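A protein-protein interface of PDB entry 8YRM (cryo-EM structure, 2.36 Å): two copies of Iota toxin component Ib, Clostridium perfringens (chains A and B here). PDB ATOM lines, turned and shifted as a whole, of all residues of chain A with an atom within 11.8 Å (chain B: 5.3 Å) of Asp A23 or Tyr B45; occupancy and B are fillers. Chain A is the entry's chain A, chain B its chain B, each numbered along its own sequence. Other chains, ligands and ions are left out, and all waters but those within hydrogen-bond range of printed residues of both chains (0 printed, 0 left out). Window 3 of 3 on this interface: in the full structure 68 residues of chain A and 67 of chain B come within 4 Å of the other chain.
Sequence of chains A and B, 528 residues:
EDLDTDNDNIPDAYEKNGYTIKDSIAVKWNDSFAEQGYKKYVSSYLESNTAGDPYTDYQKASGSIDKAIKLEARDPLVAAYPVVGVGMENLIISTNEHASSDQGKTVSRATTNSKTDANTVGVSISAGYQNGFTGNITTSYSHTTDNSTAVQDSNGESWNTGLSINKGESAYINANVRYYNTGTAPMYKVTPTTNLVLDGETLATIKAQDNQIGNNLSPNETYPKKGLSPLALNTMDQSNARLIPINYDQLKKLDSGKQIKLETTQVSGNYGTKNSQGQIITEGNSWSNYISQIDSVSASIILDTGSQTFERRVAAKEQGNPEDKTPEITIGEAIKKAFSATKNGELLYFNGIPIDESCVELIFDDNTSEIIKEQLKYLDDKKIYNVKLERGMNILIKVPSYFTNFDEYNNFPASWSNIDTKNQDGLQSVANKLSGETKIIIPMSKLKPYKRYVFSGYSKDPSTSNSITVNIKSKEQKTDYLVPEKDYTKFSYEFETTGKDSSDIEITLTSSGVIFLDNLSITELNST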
ATOM      1  N   ASN A   9     -11.568 -25.280 -35.473  1.00  0.00           N
ATOM      2  CA  ASN A   9     -10.911 -23.984 -35.379  1.00  0.00           C
ATOM      3  C   ASN A   9      -9.654 -23.891 -36.236  1.00  0.00           C
ATOM      4  O   ASN A   9      -8.883 -22.953 -36.059  1.00  0.00           O
ATOM      5  CB  ASN A   9     -10.549 -23.583 -33.952  1.00  0.00           C
ATOM      6  CG  ASN A   9     -11.759 -23.533 -33.054  1.00  0.00           C
ATOM      7  OD1 ASN A   9     -12.842 -23.133 -33.496  1.00  0.00           O
ATOM      8  ND2 ASN A   9     -11.599 -23.937 -31.802  1.00  0.00           N
ATOM      9  N   TYR A  19       0.394 -25.136 -40.996  1.00  0.00           N
ATOM     10  CA  TYR A  19      -0.043 -24.026 -40.173  1.00  0.00           C
ATOM     11  C   TYR A  19       0.711 -24.032 -38.845  1.00  0.00           C
ATOM     12  O   TYR A  19       1.354 -25.015 -38.490  1.00  0.00           O
ATOM     13  CB  TYR A  19      -1.548 -24.107 -39.937  1.00  0.00           C
ATOM     14  CG  TYR A  19      -1.971 -25.301 -39.100  1.00  0.00           C
ATOM     15  CD1 TYR A  19      -2.232 -26.537 -39.687  1.00  0.00           C
ATOM     16  CD2 TYR A  19      -2.096 -25.197 -37.723  1.00  0.00           C
ATOM     17  CE1 TYR A  19      -2.616 -27.629 -38.930  1.00  0.00           C
ATOM     18  CE2 TYR A  19      -2.468 -26.287 -36.949  1.00  0.00           C
ATOM     19  CZ  TYR A  19      -2.728 -27.505 -37.559  1.00  0.00           C
ATOM     20  OH  TYR A  19      -3.126 -28.602 -36.851  1.00  0.00           O
ATOM     21  N   THR A  20       0.632 -22.911 -38.126  1.00  0.00           N
ATOM     22  CA  THR A  20       1.156 -22.838 -36.772  1.00  0.00           C
ATOM     23  C   THR A  20       0.158 -22.066 -35.918  1.00  0.00           C
ATOM     24  O   THR A  20      -0.844 -21.573 -36.428  1.00  0.00           O
ATOM     25  CB  THR A  20       2.545 -22.198 -36.786  1.00  0.00           C
ATOM     26  OG1 THR A  20       3.176 -22.696 -35.615  1.00  0.00           O
ATOM     27  CG2 THR A  20       2.518 -20.679 -36.820  1.00  0.00           C
ATOM     28  N   ILE A  21       0.444 -21.961 -34.619  1.00  0.00           N
ATOM     29  CA  ILE A  21      -0.430 -21.246 -33.704  1.00  0.00           C
ATOM     30  C   ILE A  21       0.317 -20.043 -33.131  1.00  0.00           C
ATOM     31  O   ILE A  21       1.390 -20.198 -32.556  1.00  0.00           O
ATOM     32  CB  ILE A  21      -0.924 -22.174 -32.586  1.00  0.00           C
ATOM     33  CG1 ILE A  21      -1.506 -23.473 -33.129  1.00  0.00           C
ATOM     34  CG2 ILE A  21      -1.910 -21.446 -31.679  1.00  0.00           C
ATOM     35  CD1 ILE A  21      -2.855 -23.333 -33.799  1.00  0.00           C
ATOM     36  N   LYS A  22      -0.274 -18.853 -33.294  1.00  0.00           N
ATOM     37  CA  LYS A  22       0.247 -17.622 -32.721  1.00  0.00           C
ATOM     38  C   LYS A  22      -0.877 -16.899 -31.990  1.00  0.00           C
ATOM     39  O   LYS A  22      -1.919 -16.617 -32.583  1.00  0.00           O
ATOM     40  CB  LYS A  22       0.819 -16.707 -33.804  1.00  0.00           C
ATOM     41  CG  LYS A  22       2.117 -17.195 -34.419  1.00  0.00           C
ATOM     42  CD  LYS A  22       2.819 -16.113 -35.224  1.00  0.00           C
ATOM     43  CE  LYS A  22       4.056 -16.612 -35.902  1.00  0.00           C
ATOM     44  NZ  LYS A  22       4.886 -15.497 -36.371  1.00  0.00           N
ATOM     45  N   ASP A  23      -0.650 -16.611 -30.700  1.00  0.00           N
ATOM     46  CA  ASP A  23      -1.618 -15.936 -29.845  1.00  0.00           C
ATOM     47  C   ASP A  23      -2.951 -16.676 -29.865  1.00  0.00           C
ATOM     48  O   ASP A  23      -4.010 -16.056 -29.934  1.00  0.00           O
ATOM     49  CB  ASP A  23      -1.787 -14.474 -30.229  1.00  0.00           C
ATOM     50  CG  ASP A  23      -0.614 -13.570 -29.881  1.00  0.00           C
ATOM     51  OD1 ASP A  23       0.364 -14.071 -29.280  1.00  0.00           O
ATOM     52  OD2 ASP A  23      -0.690 -12.364 -30.206  1.00  0.00           O
ATOM     53  N   SER A  24      -2.876 -18.008 -29.805  1.00  0.00           N
ATOM     54  CA  SER A  24      -4.045 -18.867 -29.724  1.00  0.00           C
ATOM     55  C   SER A  24      -4.874 -18.834 -31.007  1.00  0.00           C
ATOM     56  O   SER A  24      -6.050 -19.181 -30.986  1.00  0.00           O
ATOM     57  CB  SER A  24      -4.884 -18.527 -28.517  1.00  0.00           C
ATOM     58  OG  SER A  24      -4.114 -18.663 -27.328  1.00  0.00           O
ATOM     59  N   ILE A  25      -4.257 -18.450 -32.125  1.00  0.00           N
ATOM     60  CA  ILE A  25      -4.943 -18.414 -33.407  1.00  0.00           C
ATOM     61  C   ILE A  25      -4.104 -19.200 -34.411  1.00  0.00           C
ATOM     62  O   ILE A  25      -2.892 -19.016 -34.492  1.00  0.00           O
ATOM     63  CB  ILE A  25      -5.158 -16.966 -33.883  1.00  0.00           C
ATOM     64  CG1 ILE A  25      -5.969 -16.147 -32.889  1.00  0.00           C
ATOM     65  CG2 ILE A  25      -5.791 -16.943 -35.270  1.00  0.00           C
ATOM     66  CD1 ILE A  25      -7.442 -16.502 -32.849  1.00  0.00           C
ATOM     67  N   ALA A  26      -4.757 -20.067 -35.182  1.00  0.00           N
ATOM     68  CA  ALA A  26      -4.083 -20.797 -36.240  1.00  0.00           C
ATOM     69  C   ALA A  26      -3.802 -19.849 -37.393  1.00  0.00           C
ATOM     70  O   ALA A  26      -4.707 -19.167 -37.864  1.00  0.00           O
ATOM     71  CB  ALA A  26      -4.914 -21.972 -36.697  1.00  0.00           C
ATOM     72  N   VAL A  27      -2.542 -19.816 -37.826  1.00  0.00           N
ATOM     73  CA  VAL A  27      -2.135 -18.960 -38.923  1.00  0.00           C
ATOM     74  C   VAL A  27      -1.441 -19.818 -39.972  1.00  0.00           C
ATOM     75  O   VAL A  27      -0.854 -20.847 -39.649  1.00  0.00           O
ATOM     76  CB  VAL A  27      -1.230 -17.807 -38.448  1.00  0.00           C
ATOM     77  CG1 VAL A  27      -1.872 -17.015 -37.316  1.00  0.00           C
ATOM     78  CG2 VAL A  27       0.138 -18.286 -38.020  1.00  0.00           C
ATOM     79  N   LYS A  28      -1.518 -19.371 -41.226  1.00  0.00           N
ATOM     80  CA  LYS A  28      -0.901 -20.075 -42.333  1.00  0.00           C
ATOM     81  C   LYS A  28       0.609 -20.103 -42.140  1.00  0.00           C
ATOM     82  O   LYS A  28       1.213 -19.081 -41.828  1.00  0.00           O
ATOM     83  CB  LYS A  28      -1.241 -19.384 -43.656  1.00  0.00           C
ATOM     84  CG  LYS A  28      -0.487 -19.926 -44.854  1.00  0.00           C
ATOM     85  CD  LYS A  28      -0.540 -19.012 -46.070  1.00  0.00           C
ATOM     86  CE  LYS A  28      -1.943 -18.715 -46.487  1.00  0.00           C
ATOM     87  NZ  LYS A  28      -1.982 -18.229 -47.869  1.00  0.00           N
ATOM     88  N   PHE A  33       9.293 -17.780 -40.286  1.00  0.00           N
ATOM     89  CA  PHE A  33       9.317 -17.903 -38.838  1.00  0.00           C
ATOM     90  C   PHE A  33       9.503 -19.357 -38.419  1.00  0.00           C
ATOM     91  O   PHE A  33       8.972 -19.784 -37.401  1.00  0.00           O
ATOM     92  CB  PHE A  33       8.077 -17.281 -38.189  1.00  0.00           C
ATOM     93  CG  PHE A  33       6.732 -17.650 -38.795  1.00  0.00           C
ATOM     94  CD1 PHE A  33       6.273 -18.957 -38.764  1.00  0.00           C
ATOM     95  CD2 PHE A  33       5.901 -16.660 -39.319  1.00  0.00           C
ATOM     96  CE1 PHE A  33       5.023 -19.267 -39.275  1.00  0.00           C
ATOM     97  CE2 PHE A  33       4.652 -16.972 -39.821  1.00  0.00           C
ATOM     98  CZ  PHE A  33       4.214 -18.274 -39.801  1.00  0.00           C
ATOM     99  N   GLN A  36      12.267 -18.850 -35.421  1.00  0.00           N
ATOM    100  CA  GLN A  36      11.818 -18.288 -34.158  1.00  0.00           C
ATOM    101  C   GLN A  36      11.258 -19.361 -33.229  1.00  0.00           C
ATOM    102  O   GLN A  36      10.756 -19.034 -32.158  1.00  0.00           O
ATOM    103  CB  GLN A  36      10.741 -17.240 -34.410  1.00  0.00           C
ATOM    104  CG  GLN A  36      11.276 -15.992 -35.097  1.00  0.00           C
ATOM    105  CD  GLN A  36      10.382 -15.510 -36.215  1.00  0.00           C
ATOM    106  OE1 GLN A  36      10.810 -15.393 -37.370  1.00  0.00           O
ATOM    107  NE2 GLN A  36       9.129 -15.228 -35.887  1.00  0.00           N
ATOM    108  N   TYR A  38       8.853 -21.698 -34.030  1.00  0.00           N
ATOM    109  CA  TYR A  38       7.544 -22.212 -34.402  1.00  0.00           C
ATOM    110  C   TYR A  38       7.705 -23.501 -35.199  1.00  0.00           C
ATOM    111  O   TYR A  38       8.662 -23.652 -35.956  1.00  0.00           O
ATOM    112  CB  TYR A  38       6.744 -21.186 -35.203  1.00  0.00           C
ATOM    113  CG  TYR A  38       6.313 -19.998 -34.364  1.00  0.00           C
ATOM    114  CD1 TYR A  38       5.200 -20.083 -33.541  1.00  0.00           C
ATOM    115  CD2 TYR A  38       7.022 -18.803 -34.385  1.00  0.00           C
ATOM    116  CE1 TYR A  38       4.801 -19.010 -32.761  1.00  0.00           C
ATOM    117  CE2 TYR A  38       6.629 -17.721 -33.616  1.00  0.00           C
ATOM    118  CZ  TYR A  38       5.514 -17.825 -32.801  1.00  0.00           C
ATOM    119  OH  TYR A  38       5.107 -16.771 -32.034  1.00  0.00           O
ATOM    120  N   LYS A  39       6.751 -24.419 -35.017  1.00  0.00           N
ATOM    121  CA  LYS A  39       6.738 -25.695 -35.718  1.00  0.00           C
ATOM    122  C   LYS A  39       5.595 -25.738 -36.731  1.00  0.00           C
ATOM    123  O   LYS A  39       4.514 -25.214 -36.477  1.00  0.00           O
ATOM    124  CB  LYS A  39       6.592 -26.828 -34.702  1.00  0.00           C
ATOM    125  CG  LYS A  39       7.785 -26.945 -33.769  1.00  0.00           C
ATOM    126  CD  LYS A  39       7.691 -28.155 -32.848  1.00  0.00           C
ATOM    127  CE  LYS A  39       9.027 -28.674 -32.414  1.00  0.00           C
ATOM    128  NZ  LYS A  39       9.608 -27.875 -31.330  1.00  0.00           N
ATOM    129  N   TYR A  41       2.679 -27.551 -38.561  1.00  0.00           N
ATOM    130  CA  TYR A  41       1.751 -28.638 -38.298  1.00  0.00           C
ATOM    131  C   TYR A  41       0.900 -28.907 -39.536  1.00  0.00           C
ATOM    132  O   TYR A  41       0.579 -27.995 -40.288  1.00  0.00           O
ATOM    133  CB  TYR A  41       0.833 -28.306 -37.125  1.00  0.00           C
ATOM    134  CG  TYR A  41       1.555 -28.089 -35.805  1.00  0.00           C
ATOM    135  CD1 TYR A  41       2.450 -29.031 -35.314  1.00  0.00           C
ATOM    136  CD2 TYR A  41       1.357 -26.929 -35.066  1.00  0.00           C
ATOM    137  CE1 TYR A  41       3.104 -28.837 -34.108  1.00  0.00           C
ATOM    138  CE2 TYR A  41       2.013 -26.717 -33.868  1.00  0.00           C
ATOM    139  CZ  TYR A  41       2.892 -27.672 -33.390  1.00  0.00           C
ATOM    140  OH  TYR A  41       3.528 -27.436 -32.202  1.00  0.00           O
ATOM    141  N   TYR A  58      -6.616 -28.645 -32.803  1.00  0.00           N
ATOM    142  CA  TYR A  58      -6.361 -27.293 -32.332  1.00  0.00           C
ATOM    143  C   TYR A  58      -5.865 -27.332 -30.888  1.00  0.00           C
ATOM    144  O   TYR A  58      -4.916 -26.633 -30.536  1.00  0.00           O
ATOM    145  CB  TYR A  58      -7.599 -26.400 -32.472  1.00  0.00           C
ATOM    146  CG  TYR A  58      -7.401 -25.060 -31.793  1.00  0.00           C
ATOM    147  CD1 TYR A  58      -6.668 -24.060 -32.415  1.00  0.00           C
ATOM    148  CD2 TYR A  58      -7.857 -24.833 -30.503  1.00  0.00           C
ATOM    149  CE1 TYR A  58      -6.423 -22.852 -31.787  1.00  0.00           C
ATOM    150  CE2 TYR A  58      -7.618 -23.627 -29.863  1.00  0.00           C
ATOM    151  CZ  TYR A  58      -6.904 -22.633 -30.509  1.00  0.00           C
ATOM    152  OH  TYR A  58      -6.677 -21.434 -29.891  1.00  0.00           O
ATOM    153  N   GLN A  59      -6.509 -28.136 -30.045  1.00  0.00           N
ATOM    154  CA  GLN A  59      -6.099 -28.220 -28.654  1.00  0.00           C
ATOM    155  C   GLN A  59      -4.640 -28.654 -28.552  1.00  0.00           C
ATOM    156  O   GLN A  59      -3.893 -28.101 -27.748  1.00  0.00           O
ATOM    157  CB  GLN A  59      -6.955 -29.194 -27.847  1.00  0.00           C
ATOM    158  CG  GLN A  59      -8.370 -28.692 -27.602  1.00  0.00           C
ATOM    159  CD  GLN A  59      -9.201 -29.691 -26.837  1.00  0.00           C
ATOM    160  OE1 GLN A  59      -9.486 -30.791 -27.315  1.00  0.00           O
ATOM    161  NE2 GLN A  59      -9.576 -29.332 -25.621  1.00  0.00           N
ATOM    162  N   ALA A  61      -2.182 -28.539 -31.015  1.00  0.00           N
ATOM    163  CA  ALA A  61      -1.261 -27.618 -31.662  1.00  0.00           C
ATOM    164  C   ALA A  61      -1.072 -26.357 -30.816  1.00  0.00           C
ATOM    165  O   ALA A  61       0.034 -25.831 -30.743  1.00  0.00           O
ATOM    166  CB  ALA A  61      -1.751 -27.280 -33.052  1.00  0.00           C
ATOM    167  N   SER A  62      -2.155 -25.878 -30.185  1.00  0.00           N
ATOM    168  CA  SER A  62      -2.134 -24.632 -29.430  1.00  0.00           C
ATOM    169  C   SER A  62      -1.620 -24.848 -28.011  1.00  0.00           C
ATOM    170  O   SER A  62      -1.398 -23.885 -27.283  1.00  0.00           O
ATOM    171  CB  SER A  62      -3.490 -24.010 -29.367  1.00  0.00           C
ATOM    172  OG  SER A  62      -4.350 -24.789 -28.548  1.00  0.00           O
ATOM    173  N   GLY A  63      -1.466 -26.110 -27.610  1.00  0.00           N
ATOM    174  CA  GLY A  63      -0.937 -26.431 -26.301  1.00  0.00           C
ATOM    175  C   GLY A  63      -1.965 -26.236 -25.192  1.00  0.00           C
ATOM    176  O   GLY A  63      -1.612 -26.273 -24.019  1.00  0.00           O
ATOM    177  N   SER A  64      -3.236 -26.052 -25.555  1.00  0.00           N
ATOM    178  CA  SER A  64      -4.277 -25.797 -24.576  1.00  0.00           C
ATOM    179  C   SER A  64      -4.785 -27.121 -24.013  1.00  0.00           C
ATOM    180  O   SER A  64      -5.980 -27.391 -24.009  1.00  0.00           O
ATOM    181  CB  SER A  64      -5.385 -24.956 -25.173  1.00  0.00           C
ATOM    182  OG  SER A  64      -6.312 -25.740 -25.907  1.00  0.00           O
ATOM    183  N   LYS A  67      -0.638 -29.723 -19.099  1.00  0.00           N
ATOM    184  CA  LYS A  67       0.727 -29.278 -19.313  1.00  0.00           C
ATOM    185  C   LYS A  67       1.722 -30.397 -19.012  1.00  0.00           C
ATOM    186  O   LYS A  67       2.888 -30.286 -19.373  1.00  0.00           O
ATOM    187  CB  LYS A  67       1.028 -28.027 -18.489  1.00  0.00           C
ATOM    188  CG  LYS A  67       0.209 -26.816 -18.881  1.00  0.00           C
ATOM    189  CD  LYS A  67       0.606 -26.261 -20.239  1.00  0.00           C
ATOM    190  CE  LYS A  67      -0.188 -25.053 -20.652  1.00  0.00           C
ATOM    191  NZ  LYS A  67      -1.625 -25.353 -20.732  1.00  0.00           N
ATOM    192  N   THR B   5      -6.896 -11.709 -24.066  1.00  0.00           N
ATOM    193  CA  THR B   5      -6.834 -12.874 -24.931  1.00  0.00           C
ATOM    194  C   THR B   5      -7.255 -14.141 -24.187  1.00  0.00           C
ATOM    195  O   THR B   5      -7.922 -14.994 -24.766  1.00  0.00           O
ATOM    196  CB  THR B   5      -5.428 -13.024 -25.496  1.00  0.00           C
ATOM    197  OG1 THR B   5      -5.148 -11.779 -26.125  1.00  0.00           O
ATOM    198  CG2 THR B   5      -5.343 -14.176 -26.481  1.00  0.00           C
ATOM    199  N   ASP B   6      -6.839 -14.277 -22.928  1.00  0.00           N
ATOM    200  CA  ASP B   6      -7.098 -15.486 -22.159  1.00  0.00           C
ATOM    201  C   ASP B   6      -8.400 -15.370 -21.370  1.00  0.00           C
ATOM    202  O   ASP B   6      -8.813 -16.344 -20.742  1.00  0.00           O
ATOM    203  CB  ASP B   6      -5.932 -15.822 -21.243  1.00  0.00           C
ATOM    204  CG  ASP B   6      -5.464 -14.699 -20.336  1.00  0.00           C
ATOM    205  OD1 ASP B   6      -6.003 -13.581 -20.452  1.00  0.00           O
ATOM    206  OD2 ASP B   6      -4.549 -14.940 -19.545  1.00  0.00           O
ATOM    207  N   ASP B  12      -4.023  -7.822 -21.637  1.00  0.00           N
ATOM    208  CA  ASP B  12      -2.743  -8.352 -22.070  1.00  0.00           C
ATOM    209  C   ASP B  12      -1.622  -7.380 -21.735  1.00  0.00           C
ATOM    210  O   ASP B  12      -0.563  -7.799 -21.279  1.00  0.00           O
ATOM    211  CB  ASP B  12      -2.761  -8.662 -23.556  1.00  0.00           C
ATOM    212  CG  ASP B  12      -3.776  -9.716 -23.961  1.00  0.00           C
ATOM    213  OD1 ASP B  12      -4.435 -10.279 -23.047  1.00  0.00           O
ATOM    214  OD2 ASP B  12      -3.893  -9.967 -25.177  1.00  0.00           O
ATOM    215  N   GLU B  15      -0.762  -7.614 -18.108  1.00  0.00           N
ATOM    216  CA  GLU B  15      -0.045  -8.825 -17.740  1.00  0.00           C
ATOM    217  C   GLU B  15       1.410  -8.771 -18.204  1.00  0.00           C
ATOM    218  O   GLU B  15       2.291  -9.185 -17.459  1.00  0.00           O
ATOM    219  CB  GLU B  15      -0.723 -10.083 -18.276  1.00  0.00           C
ATOM    220  CG  GLU B  15      -2.152 -10.252 -17.782  1.00  0.00           C
ATOM    221  CD  GLU B  15      -2.640 -11.686 -17.774  1.00  0.00           C
ATOM    222  OE1 GLU B  15      -2.041 -12.502 -17.060  1.00  0.00           O
ATOM    223  OE2 GLU B  15      -3.635 -12.001 -18.447  1.00  0.00           O
ATOM    224  N   LYS B  16       1.665  -8.270 -19.420  1.00  0.00           N
ATOM    225  CA  LYS B  16       3.022  -8.195 -19.942  1.00  0.00           C
ATOM    226  C   LYS B  16       3.859  -7.295 -19.040  1.00  0.00           C
ATOM    227  O   LYS B  16       4.922  -7.694 -18.573  1.00  0.00           O
ATOM    228  CB  LYS B  16       3.072  -7.684 -21.386  1.00  0.00           C
ATOM    229  CG  LYS B  16       2.457  -8.598 -22.430  1.00  0.00           C
ATOM    230  CD  LYS B  16       2.362  -7.945 -23.805  1.00  0.00           C
ATOM    231  CE  LYS B  16       1.290  -8.547 -24.661  1.00  0.00           C
ATOM    232  NZ  LYS B  16       0.992  -7.700 -25.820  1.00  0.00           N
ATOM    233  N   SER B  43       2.104 -11.820 -15.285  1.00  0.00           N
ATOM    234  CA  SER B  43       1.597 -13.143 -15.600  1.00  0.00           C
ATOM    235  C   SER B  43       1.536 -13.310 -17.110  1.00  0.00           C
ATOM    236  O   SER B  43       1.800 -12.372 -17.851  1.00  0.00           O
ATOM    237  CB  SER B  43       0.254 -13.410 -14.945  1.00  0.00           C
ATOM    238  OG  SER B  43      -0.564 -12.247 -14.924  1.00  0.00           O
ATOM    239  N   SER B  44       1.231 -14.525 -17.553  1.00  0.00           N
ATOM    240  CA  SER B  44       1.107 -14.802 -18.972  1.00  0.00           C
ATOM    241  C   SER B  44      -0.235 -14.297 -19.490  1.00  0.00           C
ATOM    242  O   SER B  44      -1.284 -14.626 -18.940  1.00  0.00           O
ATOM    243  CB  SER B  44       1.252 -16.260 -19.246  1.00  0.00           C
ATOM    244  OG  SER B  44       0.797 -16.559 -20.558  1.00  0.00           O
ATOM    245  N   TYR B  45      -0.197 -13.536 -20.584  1.00  0.00           N
ATOM    246  CA  TYR B  45      -1.423 -13.042 -21.178  1.00  0.00           C
ATOM    247  C   TYR B  45      -2.073 -14.110 -22.059  1.00  0.00           C
ATOM    248  O   TYR B  45      -3.180 -13.889 -22.540  1.00  0.00           O
ATOM    249  CB  TYR B  45      -1.158 -11.750 -21.949  1.00  0.00           C
ATOM    250  CG  TYR B  45      -0.402 -11.933 -23.249  1.00  0.00           C
ATOM    251  CD1 TYR B  45       0.984 -11.882 -23.275  1.00  0.00           C
ATOM    252  CD2 TYR B  45      -1.072 -12.144 -24.449  1.00  0.00           C
ATOM    253  CE1 TYR B  45       1.690 -12.042 -24.455  1.00  0.00           C
ATOM    254  CE2 TYR B  45      -0.377 -12.303 -25.639  1.00  0.00           C
ATOM    255  CZ  TYR B  45       1.006 -12.249 -25.640  1.00  0.00           C
ATOM    256  OH  TYR B  45       1.689 -12.397 -26.810  1.00  0.00           O
ATOM    257  N   LEU B  46      -1.409 -15.259 -22.242  1.00  0.00           N
ATOM    258  CA  LEU B  46      -1.966 -16.368 -23.004  1.00  0.00           C
ATOM    259  C   LEU B  46      -2.446 -17.504 -22.102  1.00  0.00           C
ATOM    260  O   LEU B  46      -3.014 -18.475 -22.592  1.00  0.00           O
ATOM    261  CB  LEU B  46      -0.946 -16.879 -24.020  1.00  0.00           C
ATOM    262  CG  LEU B  46      -0.697 -15.981 -25.239  1.00  0.00           C
ATOM    263  CD1 LEU B  46       0.209 -16.702 -26.210  1.00  0.00           C
ATOM    264  CD2 LEU B  46      -1.980 -15.538 -25.941  1.00  0.00           C
ATOM    265  N   GLU B  47      -2.226 -17.398 -20.793  1.00  0.00           N
ATOM    266  CA  GLU B  47      -2.667 -18.422 -19.860  1.00  0.00           C
ATOM    267  C   GLU B  47      -3.518 -17.793 -18.766  1.00  0.00           C
ATOM    268  O   GLU B  47      -3.130 -16.796 -18.160  1.00  0.00           O
ATOM    269  CB  GLU B  47      -1.464 -19.117 -19.227  1.00  0.00           C
ATOM    270  CG  GLU B  47      -0.952 -20.290 -20.058  1.00  0.00           C
ATOM    271  CD  GLU B  47      -1.910 -21.468 -20.092  1.00  0.00           C
ATOM    272  OE1 GLU B  47      -2.781 -21.572 -19.187  1.00  0.00           O
ATOM    273  OE2 GLU B  47      -1.799 -22.268 -21.049  1.00  0.00           O
ATOM    274  N   GLU B 323       5.618 -19.476 -27.811  1.00  0.00           N
ATOM    275  CA  GLU B 323       4.273 -19.114 -27.408  1.00  0.00           C
ATOM    276  C   GLU B 323       4.103 -19.190 -25.894  1.00  0.00           C
ATOM    277  O   GLU B 323       3.002 -18.970 -25.396  1.00  0.00           O
ATOM    278  CB  GLU B 323       3.265 -20.033 -28.096  1.00  0.00           C
ATOM    279  CG  GLU B 323       2.975 -19.625 -29.536  1.00  0.00           C
ATOM    280  CD  GLU B 323       2.371 -18.237 -29.663  1.00  0.00           C
ATOM    281  OE1 GLU B 323       1.227 -18.060 -29.185  1.00  0.00           O
ATOM    282  OE2 GLU B 323       3.046 -17.340 -30.222  1.00  0.00           O
ATOM    283  N   LYS B 325       4.484 -17.418 -22.597  1.00  0.00           N
ATOM    284  CA  LYS B 325       4.589 -16.021 -22.216  1.00  0.00           C
ATOM    285  C   LYS B 325       4.713 -15.882 -20.700  1.00  0.00           C
ATOM    286  O   LYS B 325       4.426 -14.817 -20.163  1.00  0.00           O
ATOM    287  CB  LYS B 325       3.356 -15.254 -22.698  1.00  0.00           C
ATOM    288  CG  LYS B 325       3.039 -15.413 -24.166  1.00  0.00           C
ATOM    289  CD  LYS B 325       4.164 -14.930 -25.067  1.00  0.00           C
ATOM    290  CE  LYS B 325       3.797 -15.039 -26.511  1.00  0.00           C
ATOM    291  NZ  LYS B 325       4.860 -14.464 -27.340  1.00  0.00           N
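The side-chain carboxylate (OD1) of Asp A23 lies within hydrogen-bond range of the side-chain hydroxyl (OH) of Tyr B45, 3.3 Å away. N of Asp A23 lies within hydrogen-bond range of OE1 of Glu B323. OH of Tyr A38 sits at hydrogen-bond distance from OE2 of Glu B323 (2.8 Å). NZ of Lys A67 is in salt-bridge range of OE2 of Glu B47, at 3.1 Å.
The side-chain amino group of Lys A67 sits at hydrogen-bond distance from the backbone carbonyl oxygen of Gly A63, at 3.4 Å. The side-chain hydroxyl of Ser B44 lies within hydrogen-bond range of the backbone NH of Leu B46. N of Glu B47 is in hydrogen-bond range of OG of Ser B44.
Ile A21 touches Glu B323. Lys A22 touches Glu B323. CA of Asp A23 touches CD2 of Leu B46 (3.9 Å).
No position is printed for both chains.
Printed residues of chain A that touch a printed residue of chain B: Ile A21, Lys A22, Asp A23, Tyr A38 and Lys A67. Hydrophobic or aromatic side chains of chain A that line the printed part of chain B: Tyr A38. Among the printed residues, 7 pairs touch across the chains. Among the printed residues, Asp or Glu carboxylates within 4 Å of a Lys or Arg side-chain nitrogen of the other chain: Lys A67 with Glu B47 (3.1 Å).
Of chain B, only Tyr B45 (3.3 Å), Leu B46 (3.9 Å) and Glu B323 (2.8 Å) come within 4 Å of Asp A23. Tyr B45 touches one residue of chain A. No residue of chain A comes within 4 Å of Thr B5. No residue of chain A comes within 4 Å of Asp B6. No residue of chain A comes within 4 Å of Asp B12. No residue of chain A comes within 4 Å of Glu B15. No residue of chain A comes within 4 Å of Lys B16. No residue of chain A comes within 4 Å of Ser B43. No residue of chain A comes within 4 Å of Ser B44. Leu B46 touches one residue of chain A. No residue of chain A comes within 4 Å of Lys B325. Of the printed residues of chain B, Lys A22 touches Glu B323 (3.7 Å). Of the printed residues of chain B, Lys A67 touches Glu B47. Printed residues of chain B within 4 Å of Tyr A38: Glu B323 (2.8 Å). Of the printed residues of chain B, Ile A21 touches Glu B323 (3.5 Å). Ala A26 touches none of the printed residues of chain B. Gln A59 touches none of the printed residues of chain B. The nearest residue of chain B that does not touch Asp A23 is Thr B5 (4.2 Å).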
